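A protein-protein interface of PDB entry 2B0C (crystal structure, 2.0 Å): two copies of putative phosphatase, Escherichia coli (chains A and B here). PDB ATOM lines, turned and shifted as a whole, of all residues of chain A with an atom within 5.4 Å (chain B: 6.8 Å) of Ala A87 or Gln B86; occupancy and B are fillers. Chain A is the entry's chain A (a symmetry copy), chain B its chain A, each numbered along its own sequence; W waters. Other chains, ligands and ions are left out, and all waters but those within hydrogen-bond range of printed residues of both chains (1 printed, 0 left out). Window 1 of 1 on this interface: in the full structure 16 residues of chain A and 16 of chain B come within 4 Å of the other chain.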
ATOM      1  N   ARG A  25       8.410 -13.586 -12.594  1.00  0.00           N
ATOM      2  CA  ARG A  25       8.146 -12.864 -11.355  1.00  0.00           C
ATOM      3  C   ARG A  25       7.391 -11.537 -11.631  1.00  0.00           C
ATOM      4  O   ARG A  25       6.516 -11.149 -10.872  1.00  0.00           O
ATOM      5  CB  ARG A  25       9.483 -12.639 -10.639  1.00  0.00           C
ATOM      6  CG  ARG A  25       9.425 -12.083  -9.225  1.00  0.00           C
ATOM      7  CD  ARG A  25       9.056 -13.082  -8.126  1.00  0.00           C
ATOM      8  NE  ARG A  25       9.948 -14.229  -7.890  1.00  0.00           N
ATOM      9  CZ  ARG A  25      11.106 -14.235  -7.204  1.00  0.00           C
ATOM     10  NH1 ARG A  25      11.668 -13.124  -6.717  1.00  0.00           N
ATOM     11  NH2 ARG A  25      11.743 -15.385  -7.048  1.00  0.00           N
ATOM     12  N   VAL A  26       7.731 -10.875 -12.737  1.00  0.00           N
ATOM     13  CA  VAL A  26       7.023  -9.686 -13.228  1.00  0.00           C
ATOM     14  C   VAL A  26       5.568 -10.025 -13.534  1.00  0.00           C
ATOM     15  O   VAL A  26       4.644  -9.331 -13.112  1.00  0.00           O
ATOM     16  CB  VAL A  26       7.682  -9.129 -14.513  1.00  0.00           C
ATOM     17  CG1 VAL A  26       6.879  -7.946 -15.080  1.00  0.00           C
ATOM     18  CG2 VAL A  26       9.122  -8.717 -14.244  1.00  0.00           C
ATOM     19  N   ALA A  29       3.674 -10.564 -10.370  1.00  0.00           N
ATOM     20  CA  ALA A  29       3.287  -9.268  -9.762  1.00  0.00           C
ATOM     21  C   ALA A  29       2.036  -8.675 -10.432  1.00  0.00           C
ATOM     22  O   ALA A  29       1.073  -8.258  -9.758  1.00  0.00           O
ATOM     23  CB  ALA A  29       4.449  -8.274  -9.835  1.00  0.00           C
ATOM     24  N   SER A  82       5.528  -0.354 -14.027  1.00  0.00           N
ATOM     25  CA  SER A  82       6.920  -0.204 -13.612  1.00  0.00           C
ATOM     26  C   SER A  82       7.254  -0.976 -12.320  1.00  0.00           C
ATOM     27  O   SER A  82       8.316  -1.607 -12.220  1.00  0.00           O
ATOM     28  CB  SER A  82       7.248   1.294 -13.475  1.00  0.00           C
ATOM     29  OG  SER A  82       8.585   1.518 -13.039  1.00  0.00           O
ATOM     30  N   HIS A  83       6.341  -0.924 -11.347  1.00  0.00           N
ATOM     31  CA  HIS A  83       6.465  -1.675 -10.094  1.00  0.00           C
ATOM     32  C   HIS A  83       6.580  -3.175 -10.350  1.00  0.00           C
ATOM     33  O   HIS A  83       7.443  -3.835  -9.795  1.00  0.00           O
ATOM     34  CB  HIS A  83       5.222  -1.453  -9.235  1.00  0.00           C
ATOM     35  CG  HIS A  83       5.484  -0.716  -7.973  1.00  0.00           C
ATOM     36  ND1 HIS A  83       5.443   0.659  -7.897  1.00  0.00           N
ATOM     37  CD2 HIS A  83       5.792  -1.160  -6.732  1.00  0.00           C
ATOM     38  CE1 HIS A  83       5.713   1.033  -6.658  1.00  0.00           C
ATOM     39  NE2 HIS A  83       5.929  -0.053  -5.934  1.00  0.00           N
ATOM     40  N   GLY A  84       5.682  -3.705 -11.178  1.00  0.00           N
ATOM     41  CA  GLY A  84       5.742  -5.122 -11.591  1.00  0.00           C
ATOM     42  C   GLY A  84       7.068  -5.414 -12.278  1.00  0.00           C
ATOM     43  O   GLY A  84       7.755  -6.383 -11.952  1.00  0.00           O
ATOM     44  N   TRP A  85       7.430  -4.560 -13.230  1.00  0.00           N
ATOM     45  CA  TRP A  85       8.693  -4.700 -13.985  1.00  0.00           C
ATOM     46  C   TRP A  85       9.897  -4.760 -13.040  1.00  0.00           C
ATOM     47  O   TRP A  85      10.813  -5.573 -13.225  1.00  0.00           O
ATOM     48  CB  TRP A  85       8.833  -3.505 -14.943  1.00  0.00           C
ATOM     49  CG  TRP A  85       9.658  -3.739 -16.197  1.00  0.00           C
ATOM     50  CD1 TRP A  85      10.812  -3.091 -16.550  1.00  0.00           C
ATOM     51  CD2 TRP A  85       9.352  -4.632 -17.285  1.00  0.00           C
ATOM     52  NE1 TRP A  85      11.262  -3.554 -17.768  1.00  0.00           N
ATOM     53  CE2 TRP A  85      10.387  -4.498 -18.239  1.00  0.00           C
ATOM     54  CE3 TRP A  85       8.319  -5.545 -17.532  1.00  0.00           C
ATOM     55  CZ2 TRP A  85      10.418  -5.239 -19.428  1.00  0.00           C
ATOM     56  CZ3 TRP A  85       8.359  -6.299 -18.714  1.00  0.00           C
ATOM     57  CH2 TRP A  85       9.404  -6.134 -19.644  1.00  0.00           C
ATOM     58  N   GLN A  86       9.876  -3.905 -12.017  1.00  0.00           N
ATOM     59  CA  GLN A  86      10.934  -3.854 -10.999  1.00  0.00           C
ATOM     60  C   GLN A  86      11.098  -5.166 -10.228  1.00  0.00           C
ATOM     61  O   GLN A  86      12.172  -5.430  -9.662  1.00  0.00           O
ATOM     62  CB  GLN A  86      10.652  -2.699 -10.013  1.00  0.00           C
ATOM     63  CG  GLN A  86      11.721  -2.465  -8.926  1.00  0.00           C
ATOM     64  CD  GLN A  86      13.103  -2.178  -9.493  1.00  0.00           C
ATOM     65  OE1 GLN A  86      13.880  -3.097  -9.789  1.00  0.00           O
ATOM     66  NE2 GLN A  86      13.427  -0.906  -9.622  1.00  0.00           N
ATOM     67  N   ALA A  87      10.047  -5.986 -10.212  1.00  0.00           N
ATOM     68  CA  ALA A  87      10.056  -7.254  -9.459  1.00  0.00           C
ATOM     69  C   ALA A  87      10.807  -8.371 -10.177  1.00  0.00           C
ATOM     70  O   ALA A  87      10.946  -9.469  -9.636  1.00  0.00           O
ATOM     71  CB  ALA A  87       8.627  -7.707  -9.140  1.00  0.00           C
ATOM     72  N   VAL A  88      11.294  -8.110 -11.388  1.00  0.00           N
ATOM     73  CA  VAL A  88      11.990  -9.150 -12.160  1.00  0.00           C
ATOM     74  C   VAL A  88      13.036  -9.886 -11.287  1.00  0.00           C
ATOM     75  O   VAL A  88      13.812  -9.246 -10.553  1.00  0.00           O
ATOM     76  CB  VAL A  88      12.647  -8.565 -13.436  1.00  0.00           C
ATOM     77  CG1 VAL A  88      13.808  -7.619 -13.107  1.00  0.00           C
ATOM     78  CG2 VAL A  88      13.105  -9.683 -14.384  1.00  0.00           C
ATOM     79  N   PHE A  89      13.054 -11.218 -11.361  1.00  0.00           N
ATOM     80  CA  PHE A  89      14.067 -12.002 -10.627  1.00  0.00           C
ATOM     81  C   PHE A  89      15.424 -11.891 -11.300  1.00  0.00           C
ATOM     82  O   PHE A  89      15.558 -12.139 -12.508  1.00  0.00           O
ATOM     83  CB  PHE A  89      13.676 -13.486 -10.509  1.00  0.00           C
ATOM     84  CG  PHE A  89      14.753 -14.347  -9.850  1.00  0.00           C
ATOM     85  CD1 PHE A  89      14.871 -14.390  -8.457  1.00  0.00           C
ATOM     86  CD2 PHE A  89      15.654 -15.081 -10.626  1.00  0.00           C
ATOM     87  CE1 PHE A  89      15.866 -15.163  -7.838  1.00  0.00           C
ATOM     88  CE2 PHE A  89      16.657 -15.863 -10.031  1.00  0.00           C
ATOM     89  CZ  PHE A  89      16.766 -15.908  -8.627  1.00  0.00           C
ATOM     90  N   VAL B  26      17.388  -3.551  -2.295  1.00  0.00           N
ATOM     91  CA  VAL B  26      16.536  -2.388  -2.011  1.00  0.00           C
ATOM     92  C   VAL B  26      17.392  -1.147  -1.784  1.00  0.00           C
ATOM     93  O   VAL B  26      17.153  -0.087  -2.360  1.00  0.00           O
ATOM     94  CB  VAL B  26      15.664  -2.624  -0.753  1.00  0.00           C
ATOM     95  CG1 VAL B  26      14.849  -1.368  -0.402  1.00  0.00           C
ATOM     96  CG2 VAL B  26      14.743  -3.819  -0.954  1.00  0.00           C
ATOM     97  N   PHE B  81       9.962   5.046  -2.919  1.00  0.00           N
ATOM     98  CA  PHE B  81      10.237   4.175  -1.777  1.00  0.00           C
ATOM     99  C   PHE B  81       9.781   2.759  -2.096  1.00  0.00           C
ATOM    100  O   PHE B  81      10.569   1.818  -2.002  1.00  0.00           O
ATOM    101  CB  PHE B  81       9.549   4.672  -0.503  1.00  0.00           C
ATOM    102  CG  PHE B  81       9.742   3.753   0.693  1.00  0.00           C
ATOM    103  CD1 PHE B  81      10.819   3.929   1.554  1.00  0.00           C
ATOM    104  CD2 PHE B  81       8.843   2.717   0.952  1.00  0.00           C
ATOM    105  CE1 PHE B  81      10.991   3.083   2.656  1.00  0.00           C
ATOM    106  CE2 PHE B  81       9.011   1.875   2.054  1.00  0.00           C
ATOM    107  CZ  PHE B  81      10.089   2.056   2.900  1.00  0.00           C
ATOM    108  N   SER B  82       8.506   2.638  -2.475  1.00  0.00           N
ATOM    109  CA  SER B  82       7.856   1.368  -2.791  1.00  0.00           C
ATOM    110  C   SER B  82       8.537   0.611  -3.948  1.00  0.00           C
ATOM    111  O   SER B  82       8.707  -0.614  -3.885  1.00  0.00           O
ATOM    112  CB  SER B  82       6.366   1.622  -3.082  1.00  0.00           C
ATOM    113  OG  SER B  82       5.672   0.430  -3.432  1.00  0.00           O
ATOM    114  N   HIS B  83       8.926   1.350  -4.990  1.00  0.00           N
ATOM    115  CA  HIS B  83       9.667   0.797  -6.129  1.00  0.00           C
ATOM    116  C   HIS B  83      10.975   0.151  -5.685  1.00  0.00           C
ATOM    117  O   HIS B  83      11.287  -0.959  -6.084  1.00  0.00           O
ATOM    118  CB  HIS B  83      10.019   1.917  -7.106  1.00  0.00           C
ATOM    119  CG  HIS B  83       9.343   1.804  -8.423  1.00  0.00           C
ATOM    120  ND1 HIS B  83       8.105   2.357  -8.669  1.00  0.00           N
ATOM    121  CD2 HIS B  83       9.729   1.202  -9.572  1.00  0.00           C
ATOM    122  CE1 HIS B  83       7.757   2.102  -9.918  1.00  0.00           C
ATOM    123  NE2 HIS B  83       8.725   1.402 -10.485  1.00  0.00           N
ATOM    124  N   GLY B  84      11.746   0.872  -4.873  1.00  0.00           N
ATOM    125  CA  GLY B  84      12.987   0.327  -4.287  1.00  0.00           C
ATOM    126  C   GLY B  84      12.680  -0.915  -3.465  1.00  0.00           C
ATOM    127  O   GLY B  84      13.325  -1.955  -3.615  1.00  0.00           O
ATOM    128  N   TRP B  85      11.679  -0.806  -2.599  1.00  0.00           N
ATOM    129  CA  TRP B  85      11.251  -1.925  -1.733  1.00  0.00           C
ATOM    130  C   TRP B  85      10.911  -3.166  -2.563  1.00  0.00           C
ATOM    131  O   TRP B  85      11.282  -4.293  -2.208  1.00  0.00           O
ATOM    132  CB  TRP B  85      10.024  -1.481  -0.919  1.00  0.00           C
ATOM    133  CG  TRP B  85       9.814  -2.175   0.417  1.00  0.00           C
ATOM    134  CD1 TRP B  85       8.740  -2.942   0.780  1.00  0.00           C
ATOM    135  CD2 TRP B  85      10.664  -2.103   1.577  1.00  0.00           C
ATOM    136  NE1 TRP B  85       8.889  -3.384   2.077  1.00  0.00           N
ATOM    137  CE2 TRP B  85      10.059  -2.884   2.588  1.00  0.00           C
ATOM    138  CE3 TRP B  85      11.886  -1.474   1.849  1.00  0.00           C
ATOM    139  CZ2 TRP B  85      10.630  -3.051   3.856  1.00  0.00           C
ATOM    140  CZ3 TRP B  85      12.466  -1.655   3.113  1.00  0.00           C
ATOM    141  CH2 TRP B  85      11.831  -2.436   4.097  1.00  0.00           C
ATOM    142  N   GLN B  86      10.217  -2.946  -3.681  1.00  0.00           N
ATOM    143  CA  GLN B  86       9.839  -4.019  -4.609  1.00  0.00           C
ATOM    144  C   GLN B  86      11.038  -4.764  -5.199  1.00  0.00           C
ATOM    145  O   GLN B  86      10.905  -5.917  -5.640  1.00  0.00           O
ATOM    146  CB  GLN B  86       8.969  -3.440  -5.748  1.00  0.00           C
ATOM    147  CG  GLN B  86       8.424  -4.462  -6.766  1.00  0.00           C
ATOM    148  CD  GLN B  86       7.573  -5.550  -6.128  1.00  0.00           C
ATOM    149  OE1 GLN B  86       8.087  -6.577  -5.661  1.00  0.00           O
ATOM    150  NE2 GLN B  86       6.270  -5.347  -6.129  1.00  0.00           N
ATOM    151  N   ALA B  87      12.203  -4.115  -5.200  1.00  0.00           N
ATOM    152  CA  ALA B  87      13.422  -4.698  -5.790  1.00  0.00           C
ATOM    153  C   ALA B  87      14.093  -5.726  -4.883  1.00  0.00           C
ATOM    154  O   ALA B  87      15.089  -6.337  -5.274  1.00  0.00           O
ATOM    155  CB  ALA B  87      14.423  -3.600  -6.166  1.00  0.00           C
ATOM    156  N   VAL B  88      13.566  -5.925  -3.679  1.00  0.00           N
ATOM    157  CA  VAL B  88      14.184  -6.865  -2.733  1.00  0.00           C
ATOM    158  C   VAL B  88      14.519  -8.210  -3.422  1.00  0.00           C
ATOM    159  O   VAL B  88      13.687  -8.768  -4.164  1.00  0.00           O
ATOM    160  CB  VAL B  88      13.287  -7.089  -1.488  1.00  0.00           C
ATOM    161  CG1 VAL B  88      11.992  -7.833  -1.835  1.00  0.00           C
ATOM    162  CG2 VAL B  88      14.056  -7.820  -0.377  1.00  0.00           C
ATOM    163  N   PHE B  89      15.727  -8.727  -3.186  1.00  0.00           N
ATOM    164  CA  PHE B  89      16.107 -10.042  -3.735  1.00  0.00           C
ATOM    165  C   PHE B  89      15.419 -11.163  -2.974  1.00  0.00           C
ATOM    166  O   PHE B  89      15.496 -11.233  -1.737  1.00  0.00           O
ATOM    167  CB  PHE B  89      17.630 -10.265  -3.703  1.00  0.00           C
ATOM    168  CG  PHE B  89      18.049 -11.660  -4.164  1.00  0.00           C
ATOM    169  CD1 PHE B  89      18.154 -11.954  -5.527  1.00  0.00           C
ATOM    170  CD2 PHE B  89      18.307 -12.672  -3.235  1.00  0.00           C
ATOM    171  CE1 PHE B  89      18.523 -13.236  -5.965  1.00  0.00           C
ATOM    172  CE2 PHE B  89      18.678 -13.961  -3.647  1.00  0.00           C
ATOM    173  CZ  PHE B  89      18.789 -14.248  -5.022  1.00  0.00           C
ATOM    174  N   LEU B 119       4.095  -4.052   1.341  1.00  0.00           N
ATOM    175  CA  LEU B 119       3.277  -2.865   1.182  1.00  0.00           C
ATOM    176  C   LEU B 119       2.093  -3.250   0.312  1.00  0.00           C
ATOM    177  O   LEU B 119       2.163  -4.245  -0.434  1.00  0.00           O
ATOM    178  CB  LEU B 119       4.071  -1.736   0.521  1.00  0.00           C
ATOM    179  CG  LEU B 119       5.496  -1.452   1.027  1.00  0.00           C
ATOM    180  CD1 LEU B 119       6.141  -0.373   0.186  1.00  0.00           C
ATOM    181  CD2 LEU B 119       5.581  -1.097   2.537  1.00  0.00           C
ATOM    182  N   THR B 121       1.374  -1.881  -2.232  1.00  0.00           N
ATOM    183  CA  THR B 121       1.839  -1.654  -3.601  1.00  0.00           C
ATOM    184  C   THR B 121       2.863  -2.681  -4.111  1.00  0.00           C
ATOM    185  O   THR B 121       3.289  -2.606  -5.271  1.00  0.00           O
ATOM    186  CB  THR B 121       2.448  -0.229  -3.755  1.00  0.00           C
ATOM    187  OG1 THR B 121       3.278   0.066  -2.616  1.00  0.00           O
ATOM    188  CG2 THR B 121       1.334   0.830  -3.851  1.00  0.00           C
ATOM    189  N   THR B 122       3.261  -3.630  -3.259  1.00  0.00           N
ATOM    190  CA  THR B 122       4.321  -4.570  -3.630  1.00  0.00           C
ATOM    191  C   THR B 122       3.833  -6.011  -3.715  1.00  0.00           C
ATOM    192  O   THR B 122       2.928  -6.436  -2.975  1.00  0.00           O
ATOM    193  CB  THR B 122       5.552  -4.498  -2.693  1.00  0.00           C
ATOM    194  OG1 THR B 122       5.133  -4.737  -1.348  1.00  0.00           O
ATOM    195  CG2 THR B 122       6.218  -3.132  -2.760  1.00  0.00           C
ATOM    196  N   PHE B 123       4.413  -6.738  -4.662  1.00  0.00           N
ATOM    197  CA  PHE B 123       4.309  -8.188  -4.747  1.00  0.00           C
ATOM    198  C   PHE B 123       5.393  -8.793  -3.861  1.00  0.00           C
ATOM    199  O   PHE B 123       6.578  -8.647  -4.154  1.00  0.00           O
ATOM    200  CB  PHE B 123       4.537  -8.598  -6.197  1.00  0.00           C
ATOM    201  CG  PHE B 123       4.347 -10.067  -6.473  1.00  0.00           C
ATOM    202  CD1 PHE B 123       3.227 -10.751  -5.997  1.00  0.00           C
ATOM    203  CD2 PHE B 123       5.276 -10.757  -7.255  1.00  0.00           C
ATOM    204  CE1 PHE B 123       3.038 -12.119  -6.283  1.00  0.00           C
ATOM    205  CE2 PHE B 123       5.089 -12.121  -7.556  1.00  0.00           C
ATOM    206  CZ  PHE B 123       3.965 -12.792  -7.063  1.00  0.00           C
ATOM    207  N   TRP B 124       4.973  -9.479  -2.795  1.00  0.00           N
ATOM    208  CA  TRP B 124       5.854  -9.937  -1.716  1.00  0.00           C
ATOM    209  C   TRP B 124       5.841 -11.476  -1.635  1.00  0.00           C
ATOM    210  O   TRP B 124       4.847 -12.096  -2.056  1.00  0.00           O
ATOM    211  CB  TRP B 124       5.361  -9.306  -0.391  1.00  0.00           C
ATOM    212  CG  TRP B 124       6.474  -8.763   0.491  1.00  0.00           C
ATOM    213  CD1 TRP B 124       6.753  -9.133   1.781  1.00  0.00           C
ATOM    214  CD2 TRP B 124       7.456  -7.787   0.132  1.00  0.00           C
ATOM    215  NE1 TRP B 124       7.840  -8.448   2.244  1.00  0.00           N
ATOM    216  CE2 TRP B 124       8.293  -7.607   1.258  1.00  0.00           C
ATOM    217  CE3 TRP B 124       7.709  -7.038  -1.029  1.00  0.00           C
ATOM    218  CZ2 TRP B 124       9.370  -6.720   1.256  1.00  0.00           C
ATOM    219  CZ3 TRP B 124       8.778  -6.152  -1.028  1.00  0.00           C
ATOM    220  CH2 TRP B 124       9.596  -6.001   0.107  1.00  0.00           C
ATOM    221  N   TYR B 128       3.552 -15.269  -3.379  1.00  0.00           N
ATOM    222  CA  TYR B 128       4.058 -16.076  -4.478  1.00  0.00           C
ATOM    223  C   TYR B 128       3.221 -17.336  -4.542  1.00  0.00           C
ATOM    224  O   TYR B 128       2.979 -17.975  -3.507  1.00  0.00           O
ATOM    225  CB  TYR B 128       5.526 -16.472  -4.278  1.00  0.00           C
ATOM    226  CG  TYR B 128       6.574 -15.374  -4.394  1.00  0.00           C
ATOM    227  CD1 TYR B 128       6.229 -14.015  -4.557  1.00  0.00           C
ATOM    228  CD2 TYR B 128       7.927 -15.703  -4.315  1.00  0.00           C
ATOM    229  CE1 TYR B 128       7.227 -13.019  -4.648  1.00  0.00           C
ATOM    230  CE2 TYR B 128       8.908 -14.731  -4.395  1.00  0.00           C
ATOM    231  CZ  TYR B 128       8.563 -13.402  -4.567  1.00  0.00           C
ATOM    232  OH  TYR B 128       9.572 -12.484  -4.631  1.00  0.00           O
HETATM  233  O   HOH W   1      13.871 -10.874  -6.272  1.00  0.00           O
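His A83 touches its own counterpart, His B83.
His A83 touches Gln B86, and with the chains exchanged Gln A86 touches His B83.
Gln A86 touches Ala B87, and with the chains exchanged Ala A87 touches Gln B86.
Phe A89 touches its own counterpart, Phe B89.
Positions printed for both chains: 26, 82, 83, 84, 85, 86, 87, 88 and 89.
Among the printed residues, pairs that only touch across the chains: His A83 with Thr B121 (3.2 Å), His A83 with Gln B86 (3.2 Å), Gln A86 with His B83 (3.2 Å), Ala A29 with Phe B123 (3.5 Å), Ala A87 with Gln B86 (3.7 Å), Gln A86 with Ala B87 (3.7 Å), Arg A25 with Phe B123 (3.7 Å) and Phe A89 with Phe B89 (3.8 Å).
The side-chain hydroxyl of Ser B82 lies within hydrogen-bond range of a ring nitrogen (NE2) of His A83 (2.6 Å).
OH of Tyr B128 sits at hydrogen-bond distance from NH1 of Arg A25 (3.0 Å).
NE2 of His B83 sits at hydrogen-bond distance from OG of Ser A82.
A ring nitrogen (ND1) of His A83 lies within hydrogen-bond range of a ring nitrogen (ND1) of His B83, at 3.3 Å.
Of the printed residues of chain B, Arg A25 touches Phe B123 (3.7 Å) and Tyr B128 (3.0 Å).
Of the printed residues of chain B, Ala A29 touches Phe B123 (3.5 Å).
Gln B86 touches just these residues of chain A: His A83 and Ala A87.
Of the printed residues of chain A, Thr B121 touches His A83 (3.2 Å).
Of the printed residues of chain A, Phe B123 touches Arg A25 and Ala A29.
The nearest residue of chain A that does not touch Gln B86 is Gln A86 (4.2 Å).
The nearest printed residue of chain B that does not touch Ser A82 is Gln B86 (6.2 Å).
Of the 16 printed residues of chain B, 8 touch a printed residue of chain A.
Hydrophobic or aromatic side chains of chain B within 4 Å of the printed part of chain A: His B83, Ala B87, Phe B89, Phe B123 and Tyr B128.
Along chain B the printed residues that touch a printed residue of chain A span positions 82 to 128.
Printed residues of chain A that touch a printed residue of chain B: Arg A25, Ala A29, Ser A82, His A83, Gln A86, Ala A87 and Phe A89.
Along chain A the printed residues that touch a printed residue of chain B span positions 25 to 89.
Among the printed residues, no Asp or Glu carboxylate lies within 4 Å of a Lys or Arg side-chain nitrogen of the other chain.
Water W1 bridges the backbone carbonyl oxygen (O) of Val B88 and the guanidinium group (NH1) of Arg A25.
NE2 of Gln B86 lies close to N of Phe B123.
The side-chain hydroxyl of Ser B82 is in hydrogen-bond range of the side-chain hydroxyl of Thr B121 (2.6 Å).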
